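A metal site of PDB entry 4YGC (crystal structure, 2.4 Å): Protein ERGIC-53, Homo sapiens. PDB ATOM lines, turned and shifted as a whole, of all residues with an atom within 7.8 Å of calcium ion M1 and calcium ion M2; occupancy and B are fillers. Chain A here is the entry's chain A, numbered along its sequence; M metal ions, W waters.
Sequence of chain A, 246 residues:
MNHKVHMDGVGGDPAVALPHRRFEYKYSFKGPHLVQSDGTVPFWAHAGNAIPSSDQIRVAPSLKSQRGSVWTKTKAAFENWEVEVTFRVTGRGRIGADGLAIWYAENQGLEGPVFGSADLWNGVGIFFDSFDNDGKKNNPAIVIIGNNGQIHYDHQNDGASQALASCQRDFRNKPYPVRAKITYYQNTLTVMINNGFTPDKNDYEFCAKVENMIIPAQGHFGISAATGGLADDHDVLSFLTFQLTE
The backbone carbonyl oxygen (O) of Asp 129 sits at hydrogen-bond distance from the side-chain amide nitrogen (ND2) of Asn 139 (3.3 Å). The backbone NH (N) of Asp 129 lies within hydrogen-bond range of the backbone carbonyl oxygen (O) of Ala 141 (2.8 Å). O of Phe 131 sits close to ND2 of Asn 139. The side-chain carboxylate (OD2) of Asp 132 is in hydrogen-bond range of the backbone NH (N) of Lys 136, 3.0 Å away. OD1 of Asp 132 lies close to N of Gly 135, 3.3 Å away. The side-chain carboxylate (OD2) of Asp 132 sits at hydrogen-bond distance from the backbone NH (N) of Lys 137. The backbone NH (N) of Asn 139 lies close to the side-chain amide nitrogen (NE2) of Gln 168 (3.4 Å). O of Gln 156 sits at hydrogen-bond distance from N of Asp 134, 3.3 Å away.
Along chain A the residues within 4 Å of calcium ion M1 span positions 132 to 158.
Four residues have an atom within 4 Å of calcium ion M2: Asp 129, Phe 131, Asn 133 and Asp 158.
Calcium ion M1 is bound by OD2 of Asp 158 (2.3 Å), OD1 of Asn 138 (2.3 Å), OD1 of Asp 132 (2.4 Å), OD1 of Asn 139 (2.5 Å) and OD1 of Asp 134 (2.5 Å). Calcium ion M1 has five donor atoms within binding distance.
OD1 of Asp 158 binds calcium ion M2, 2.2 Å away. Calcium ion M2 is bound by the side-chain carboxylate (OD1) of Asp 129, 2.3 Å away. Calcium ion M2 is bound by the side-chain amide oxygen (OD1) of Asn 133 (2.3 Å). Water W2 is bound to calcium ion M2 (2.3 Å). Calcium ion M2 is bound by water W1. Calcium ion M2 is bound by O of Phe 131. OD2 of Asp 129 binds calcium ion M2 (2.5 Å).
Water W1 lies within hydrogen-bond range of the side-chain hydroxyl (OH) of Tyr 153 (3.0 Å) and the backbone carbonyl oxygen (O) of His 155 (3.0 Å).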
ATOM      1  N   GLY A  96      17.609 -14.663 -16.644  1.00  0.00           N
ATOM      2  CA  GLY A  96      16.391 -14.213 -17.302  1.00  0.00           C
ATOM      3  C   GLY A  96      15.826 -15.283 -18.247  1.00  0.00           C
ATOM      4  O   GLY A  96      16.426 -16.325 -18.427  1.00  0.00           O
ATOM      5  N   ALA A  97      14.662 -15.010 -18.817  1.00  0.00           N
ATOM      6  CA  ALA A  97      13.909 -15.981 -19.590  1.00  0.00           C
ATOM      7  C   ALA A  97      13.022 -15.288 -20.629  1.00  0.00           C
ATOM      8  O   ALA A  97      12.634 -14.131 -20.381  1.00  0.00           O
ATOM      9  CB  ALA A  97      13.061 -16.803 -18.654  1.00  0.00           C
ATOM     10  N   ASP A  98      12.660 -15.937 -21.758  1.00  0.00           N
ATOM     11  CA  ASP A  98      13.110 -17.253 -22.165  1.00  0.00           C
ATOM     12  C   ASP A  98      14.144 -17.177 -23.245  1.00  0.00           C
ATOM     13  O   ASP A  98      15.065 -17.993 -23.304  1.00  0.00           O
ATOM     14  CB  ASP A  98      11.947 -18.115 -22.685  1.00  0.00           C
ATOM     15  CG  ASP A  98      11.247 -18.848 -21.591  1.00  0.00           C
ATOM     16  OD1 ASP A  98      10.099 -18.517 -21.272  1.00  0.00           O
ATOM     17  OD2 ASP A  98      11.902 -19.658 -20.923  1.00  0.00           O
ATOM     18  N   GLY A  99      14.013 -16.158 -24.092  1.00  0.00           N
ATOM     19  CA  GLY A  99      14.995 -15.913 -25.119  1.00  0.00           C
ATOM     20  C   GLY A  99      14.321 -15.475 -26.374  1.00  0.00           C
ATOM     21  O   GLY A  99      13.150 -15.163 -26.411  1.00  0.00           O
ATOM     22  N   PHE A 115       9.505 -20.068 -28.363  1.00  0.00           N
ATOM     23  CA  PHE A 115       9.963 -18.698 -28.222  1.00  0.00           C
ATOM     24  C   PHE A 115       8.987 -17.766 -28.871  1.00  0.00           C
ATOM     25  O   PHE A 115       9.389 -16.810 -29.580  1.00  0.00           O
ATOM     26  CB  PHE A 115      11.352 -18.562 -28.815  1.00  0.00           C
ATOM     27  CG  PHE A 115      12.410 -19.321 -28.079  1.00  0.00           C
ATOM     28  CD1 PHE A 115      12.971 -18.790 -26.945  1.00  0.00           C
ATOM     29  CD2 PHE A 115      12.795 -20.563 -28.495  1.00  0.00           C
ATOM     30  CE1 PHE A 115      13.919 -19.494 -26.220  1.00  0.00           C
ATOM     31  CE2 PHE A 115      13.773 -21.266 -27.791  1.00  0.00           C
ATOM     32  CZ  PHE A 115      14.326 -20.726 -26.649  1.00  0.00           C
ATOM     33  N   PHE A 128      18.200 -18.211 -29.219  1.00  0.00           N
ATOM     34  CA  PHE A 128      19.067 -17.532 -28.230  1.00  0.00           C
ATOM     35  C   PHE A 128      18.362 -17.768 -26.923  1.00  0.00           C
ATOM     36  O   PHE A 128      17.411 -17.067 -26.607  1.00  0.00           O
ATOM     37  CB  PHE A 128      19.201 -16.042 -28.551  1.00  0.00           C
ATOM     38  CG  PHE A 128      19.869 -15.791 -29.850  1.00  0.00           C
ATOM     39  CD1 PHE A 128      21.135 -15.264 -29.895  1.00  0.00           C
ATOM     40  CD2 PHE A 128      19.250 -16.161 -31.045  1.00  0.00           C
ATOM     41  CE1 PHE A 128      21.773 -15.069 -31.098  1.00  0.00           C
ATOM     42  CE2 PHE A 128      19.869 -15.954 -32.253  1.00  0.00           C
ATOM     43  CZ  PHE A 128      21.146 -15.430 -32.285  1.00  0.00           C
ATOM     44  N   ASP A 129      18.791 -18.810 -26.230  1.00  0.00           N
ATOM     45  CA  ASP A 129      18.038 -19.374 -25.096  1.00  0.00           C
ATOM     46  C   ASP A 129      18.647 -18.877 -23.795  1.00  0.00           C
ATOM     47  O   ASP A 129      19.758 -19.264 -23.464  1.00  0.00           O
ATOM     48  CB  ASP A 129      18.050 -20.898 -25.154  1.00  0.00           C
ATOM     49  CG  ASP A 129      17.118 -21.561 -24.136  1.00  0.00           C
ATOM     50  OD1 ASP A 129      16.547 -20.883 -23.240  1.00  0.00           O
ATOM     51  OD2 ASP A 129      16.932 -22.778 -24.217  1.00  0.00           O
ATOM     52  N   SER A 130      17.939 -18.013 -23.084  1.00  0.00           N
ATOM     53  CA  SER A 130      18.458 -17.405 -21.860  1.00  0.00           C
ATOM     54  C   SER A 130      18.377 -18.314 -20.657  1.00  0.00           C
ATOM     55  O   SER A 130      19.194 -18.214 -19.756  1.00  0.00           O
ATOM     56  CB  SER A 130      17.608 -16.222 -21.477  1.00  0.00           C
ATOM     57  OG  SER A 130      17.409 -15.301 -22.520  1.00  0.00           O
ATOM     58  N   PHE A 131      17.323 -19.130 -20.596  1.00  0.00           N
ATOM     59  CA  PHE A 131      16.961 -19.831 -19.376  1.00  0.00           C
ATOM     60  C   PHE A 131      17.239 -21.315 -19.435  1.00  0.00           C
ATOM     61  O   PHE A 131      16.838 -22.024 -20.369  1.00  0.00           O
ATOM     62  CB  PHE A 131      15.490 -19.615 -19.060  1.00  0.00           C
ATOM     63  CG  PHE A 131      15.082 -20.216 -17.756  1.00  0.00           C
ATOM     64  CD1 PHE A 131      15.476 -19.614 -16.552  1.00  0.00           C
ATOM     65  CD2 PHE A 131      14.314 -21.394 -17.712  1.00  0.00           C
ATOM     66  CE1 PHE A 131      15.143 -20.192 -15.326  1.00  0.00           C
ATOM     67  CE2 PHE A 131      13.954 -21.951 -16.485  1.00  0.00           C
ATOM     68  CZ  PHE A 131      14.357 -21.358 -15.288  1.00  0.00           C
ATOM     69  N   ASP A 132      17.963 -21.774 -18.416  1.00  0.00           N
ATOM     70  CA  ASP A 132      18.481 -23.124 -18.308  1.00  0.00           C
ATOM     71  C   ASP A 132      17.388 -24.073 -17.773  1.00  0.00           C
ATOM     72  O   ASP A 132      17.388 -24.439 -16.617  1.00  0.00           O
ATOM     73  CB  ASP A 132      19.674 -23.083 -17.360  1.00  0.00           C
ATOM     74  CG  ASP A 132      20.428 -24.383 -17.309  1.00  0.00           C
ATOM     75  OD1 ASP A 132      20.313 -25.187 -18.238  1.00  0.00           O
ATOM     76  OD2 ASP A 132      21.187 -24.543 -16.331  1.00  0.00           O
ATOM     77  N   ASN A 133      16.468 -24.456 -18.645  1.00  0.00           N
ATOM     78  CA  ASN A 133      15.305 -25.286 -18.279  1.00  0.00           C
ATOM     79  C   ASN A 133      15.691 -26.680 -17.739  1.00  0.00           C
ATOM     80  O   ASN A 133      14.930 -27.280 -16.990  1.00  0.00           O
ATOM     81  CB  ASN A 133      14.375 -25.445 -19.492  1.00  0.00           C
ATOM     82  CG  ASN A 133      13.584 -24.188 -19.807  1.00  0.00           C
ATOM     83  OD1 ASN A 133      13.949 -23.375 -20.680  1.00  0.00           O
ATOM     84  ND2 ASN A 133      12.437 -24.036 -19.116  1.00  0.00           N
ATOM     85  N   ASP A 134      16.811 -27.208 -18.203  1.00  0.00           N
ATOM     86  CA  ASP A 134      17.320 -28.503 -17.752  1.00  0.00           C
ATOM     87  C   ASP A 134      18.354 -28.422 -16.601  1.00  0.00           C
ATOM     88  O   ASP A 134      18.833 -29.441 -16.155  1.00  0.00           O
ATOM     89  CB  ASP A 134      17.894 -29.311 -18.939  1.00  0.00           C
ATOM     90  CG  ASP A 134      18.961 -28.584 -19.707  1.00  0.00           C
ATOM     91  OD1 ASP A 134      19.305 -27.427 -19.313  1.00  0.00           O
ATOM     92  OD2 ASP A 134      19.478 -29.128 -20.708  1.00  0.00           O
ATOM     93  N   GLY A 135      18.718 -27.229 -16.149  1.00  0.00           N
ATOM     94  CA  GLY A 135      19.653 -27.079 -15.049  1.00  0.00           C
ATOM     95  C   GLY A 135      21.063 -27.577 -15.267  1.00  0.00           C
ATOM     96  O   GLY A 135      21.714 -27.986 -14.329  1.00  0.00           O
ATOM     97  N   LYS A 136      21.534 -27.568 -16.499  1.00  0.00           N
ATOM     98  CA  LYS A 136      22.905 -28.002 -16.805  1.00  0.00           C
ATOM     99  C   LYS A 136      23.949 -26.887 -16.722  1.00  0.00           C
ATOM    100  O   LYS A 136      25.081 -27.093 -17.146  1.00  0.00           O
ATOM    101  CB  LYS A 136      22.944 -28.612 -18.207  1.00  0.00           C
ATOM    102  CG  LYS A 136      21.919 -29.717 -18.439  1.00  0.00           C
ATOM    103  CD  LYS A 136      22.372 -31.099 -18.155  1.00  0.00           C
ATOM    104  CE  LYS A 136      21.548 -31.903 -19.166  1.00  0.00           C
ATOM    105  NZ  LYS A 136      22.263 -32.033 -20.465  1.00  0.00           N
ATOM    106  N   LYS A 137      23.543 -25.701 -16.252  1.00  0.00           N
ATOM    107  CA  LYS A 137      24.455 -24.543 -16.122  1.00  0.00           C
ATOM    108  C   LYS A 137      25.214 -24.246 -17.441  1.00  0.00           C
ATOM    109  O   LYS A 137      26.409 -23.995 -17.458  1.00  0.00           O
ATOM    110  CB  LYS A 137      25.360 -24.676 -14.889  1.00  0.00           C
ATOM    111  CG  LYS A 137      24.602 -24.280 -13.624  1.00  0.00           C
ATOM    112  CD  LYS A 137      24.989 -24.988 -12.352  1.00  0.00           C
ATOM    113  CE  LYS A 137      23.865 -24.868 -11.302  1.00  0.00           C
ATOM    114  NZ  LYS A 137      24.347 -24.395  -9.964  1.00  0.00           N
ATOM    115  N   ASN A 138      24.485 -24.297 -18.553  1.00  0.00           N
ATOM    116  CA  ASN A 138      25.048 -24.101 -19.874  1.00  0.00           C
ATOM    117  C   ASN A 138      24.154 -23.109 -20.648  1.00  0.00           C
ATOM    118  O   ASN A 138      23.814 -23.340 -21.811  1.00  0.00           O
ATOM    119  CB  ASN A 138      25.101 -25.454 -20.603  1.00  0.00           C
ATOM    120  CG  ASN A 138      23.744 -26.091 -20.711  1.00  0.00           C
ATOM    121  OD1 ASN A 138      22.845 -25.759 -19.950  1.00  0.00           O
ATOM    122  ND2 ASN A 138      23.592 -27.016 -21.647  1.00  0.00           N
ATOM    123  N   ASN A 139      23.792 -22.023 -19.980  1.00  0.00           N
ATOM    124  CA  ASN A 139      23.060 -20.924 -20.587  1.00  0.00           C
ATOM    125  C   ASN A 139      23.649 -19.599 -20.153  1.00  0.00           C
ATOM    126  O   ASN A 139      24.233 -19.549 -19.089  1.00  0.00           O
ATOM    127  CB  ASN A 139      21.607 -21.007 -20.175  1.00  0.00           C
ATOM    128  CG  ASN A 139      20.936 -22.225 -20.751  1.00  0.00           C
ATOM    129  OD1 ASN A 139      21.198 -23.339 -20.307  1.00  0.00           O
ATOM    130  ND2 ASN A 139      20.053 -22.023 -21.725  1.00  0.00           N
ATOM    131  N   PRO A 140      23.447 -18.496 -20.924  1.00  0.00           N
ATOM    132  CA  PRO A 140      22.686 -18.445 -22.171  1.00  0.00           C
ATOM    133  C   PRO A 140      23.391 -19.187 -23.257  1.00  0.00           C
ATOM    134  O   PRO A 140      24.594 -19.318 -23.225  1.00  0.00           O
ATOM    135  CB  PRO A 140      22.639 -16.936 -22.496  1.00  0.00           C
ATOM    136  CG  PRO A 140      22.746 -16.261 -21.170  1.00  0.00           C
ATOM    137  CD  PRO A 140      23.728 -17.135 -20.412  1.00  0.00           C
ATOM    138  N   ALA A 141      22.626 -19.688 -24.223  1.00  0.00           N
ATOM    139  CA  ALA A 141      23.171 -20.555 -25.271  1.00  0.00           C
ATOM    140  C   ALA A 141      22.536 -20.210 -26.589  1.00  0.00           C
ATOM    141  O   ALA A 141      21.411 -19.741 -26.624  1.00  0.00           O
ATOM    142  CB  ALA A 141      22.850 -22.010 -24.952  1.00  0.00           C
ATOM    143  N   TYR A 153       9.587 -29.099 -30.538  1.00  0.00           N
ATOM    144  CA  TYR A 153      10.728 -28.497 -29.812  1.00  0.00           C
ATOM    145  C   TYR A 153      10.724 -28.958 -28.357  1.00  0.00           C
ATOM    146  O   TYR A 153       9.700 -28.857 -27.650  1.00  0.00           O
ATOM    147  CB  TYR A 153      10.670 -26.977 -29.874  1.00  0.00           C
ATOM    148  CG  TYR A 153      11.632 -26.280 -28.949  1.00  0.00           C
ATOM    149  CD1 TYR A 153      13.005 -26.454 -29.092  1.00  0.00           C
ATOM    150  CD2 TYR A 153      11.172 -25.445 -27.918  1.00  0.00           C
ATOM    151  CE1 TYR A 153      13.897 -25.831 -28.234  1.00  0.00           C
ATOM    152  CE2 TYR A 153      12.067 -24.763 -27.099  1.00  0.00           C
ATOM    153  CZ  TYR A 153      13.413 -24.959 -27.257  1.00  0.00           C
ATOM    154  OH  TYR A 153      14.295 -24.334 -26.413  1.00  0.00           O
ATOM    155  N   ASP A 154      11.864 -29.459 -27.906  1.00  0.00           N
ATOM    156  CA  ASP A 154      12.067 -29.948 -26.555  1.00  0.00           C
ATOM    157  C   ASP A 154      12.384 -28.801 -25.567  1.00  0.00           C
ATOM    158  O   ASP A 154      13.524 -28.620 -25.120  1.00  0.00           O
ATOM    159  CB  ASP A 154      13.230 -30.975 -26.552  1.00  0.00           C
ATOM    160  CG  ASP A 154      13.277 -31.824 -25.269  1.00  0.00           C
ATOM    161  OD1 ASP A 154      12.461 -31.600 -24.338  1.00  0.00           O
ATOM    162  OD2 ASP A 154      14.184 -32.682 -25.167  1.00  0.00           O
ATOM    163  N   HIS A 155      11.372 -28.006 -25.267  1.00  0.00           N
ATOM    164  CA  HIS A 155      11.513 -26.858 -24.376  1.00  0.00           C
ATOM    165  C   HIS A 155      12.210 -27.153 -23.050  1.00  0.00           C
ATOM    166  O   HIS A 155      13.165 -26.468 -22.663  1.00  0.00           O
ATOM    167  CB  HIS A 155      10.144 -26.236 -24.073  1.00  0.00           C
ATOM    168  CG  HIS A 155      10.226 -24.912 -23.377  1.00  0.00           C
ATOM    169  ND1 HIS A 155      10.618 -23.740 -24.003  1.00  0.00           N
ATOM    170  CD2 HIS A 155      10.019 -24.578 -22.073  1.00  0.00           C
ATOM    171  CE1 HIS A 155      10.630 -22.751 -23.119  1.00  0.00           C
ATOM    172  NE2 HIS A 155      10.266 -23.232 -21.944  1.00  0.00           N
ATOM    173  N   GLN A 156      11.782 -28.173 -22.371  1.00  0.00           N
ATOM    174  CA  GLN A 156      12.300 -28.450 -21.020  1.00  0.00           C
ATOM    175  C   GLN A 156      13.806 -28.868 -20.980  1.00  0.00           C
ATOM    176  O   GLN A 156      14.436 -28.791 -19.937  1.00  0.00           O
ATOM    177  CB  GLN A 156      11.335 -29.402 -20.281  1.00  0.00           C
ATOM    178  CG  GLN A 156      11.754 -30.855 -20.291  1.00  0.00           C
ATOM    179  CD  GLN A 156      10.622 -31.878 -20.247  1.00  0.00           C
ATOM    180  OE1 GLN A 156      10.868 -33.105 -20.214  1.00  0.00           O
ATOM    181  NE2 GLN A 156       9.377 -31.386 -20.329  1.00  0.00           N
ATOM    182  N   ASN A 157      14.371 -29.269 -22.130  1.00  0.00           N
ATOM    183  CA  ASN A 157      15.801 -29.605 -22.212  1.00  0.00           C
ATOM    184  C   ASN A 157      16.590 -28.642 -23.083  1.00  0.00           C
ATOM    185  O   ASN A 157      17.693 -28.970 -23.556  1.00  0.00           O
ATOM    186  CB  ASN A 157      15.977 -31.035 -22.713  1.00  0.00           C
ATOM    187  CG  ASN A 157      15.314 -32.038 -21.768  1.00  0.00           C
ATOM    188  OD1 ASN A 157      15.762 -32.229 -20.638  1.00  0.00           O
ATOM    189  ND2 ASN A 157      14.243 -32.634 -22.219  1.00  0.00           N
ATOM    190  N   ASP A 158      16.014 -27.446 -23.298  1.00  0.00           N
ATOM    191  CA  ASP A 158      16.637 -26.404 -24.133  1.00  0.00           C
ATOM    192  C   ASP A 158      17.027 -26.964 -25.509  1.00  0.00           C
ATOM    193  O   ASP A 158      18.043 -26.579 -26.047  1.00  0.00           O
ATOM    194  CB  ASP A 158      17.895 -25.776 -23.443  1.00  0.00           C
ATOM    195  CG  ASP A 158      17.609 -25.122 -22.078  1.00  0.00           C
ATOM    196  OD1 ASP A 158      16.520 -24.514 -21.893  1.00  0.00           O
ATOM    197  OD2 ASP A 158      18.458 -25.282 -21.199  1.00  0.00           O
ATOM    198  N   GLY A 159      16.196 -27.850 -26.057  1.00  0.00           N
ATOM    199  CA  GLY A 159      16.431 -28.474 -27.342  1.00  0.00           C
ATOM    200  C   GLY A 159      17.758 -29.159 -27.513  1.00  0.00           C
ATOM    201  O   GLY A 159      18.212 -29.377 -28.637  1.00  0.00           O
ATOM    202  N   ALA A 160      18.403 -29.525 -26.410  1.00  0.00           N
ATOM    203  CA  ALA A 160      19.762 -30.034 -26.486  1.00  0.00           C
ATOM    204  C   ALA A 160      19.928 -31.279 -27.401  1.00  0.00           C
ATOM    205  O   ALA A 160      20.970 -31.447 -28.014  1.00  0.00           O
ATOM    206  CB  ALA A 160      20.299 -30.324 -25.086  1.00  0.00           C
ATOM    207  N   GLN A 168      27.896 -21.448 -26.254  1.00  0.00           N
ATOM    208  CA  GLN A 168      27.600 -20.727 -25.026  1.00  0.00           C
ATOM    209  C   GLN A 168      27.995 -19.274 -25.226  1.00  0.00           C
ATOM    210  O   GLN A 168      29.111 -18.972 -25.579  1.00  0.00           O
ATOM    211  CB  GLN A 168      28.326 -21.377 -23.840  1.00  0.00           C
ATOM    212  CG  GLN A 168      27.590 -22.611 -23.283  1.00  0.00           C
ATOM    213  CD  GLN A 168      27.641 -22.659 -21.771  1.00  0.00           C
ATOM    214  OE1 GLN A 168      28.270 -23.532 -21.163  1.00  0.00           O
ATOM    215  NE2 GLN A 168      27.005 -21.690 -21.155  1.00  0.00           N
HETATM  216 CA    CA M   1      20.605 -25.702 -20.588  1.00  0.00          CA
HETATM  217 CA    CA M   2      15.497 -22.607 -22.224  1.00  0.00          CA
HETATM  218  O   HOH W   1      13.893 -23.689 -23.559  1.00  0.00           O
HETATM  219  O   HOH W   2      14.094 -20.762 -22.391  1.00  0.00           O
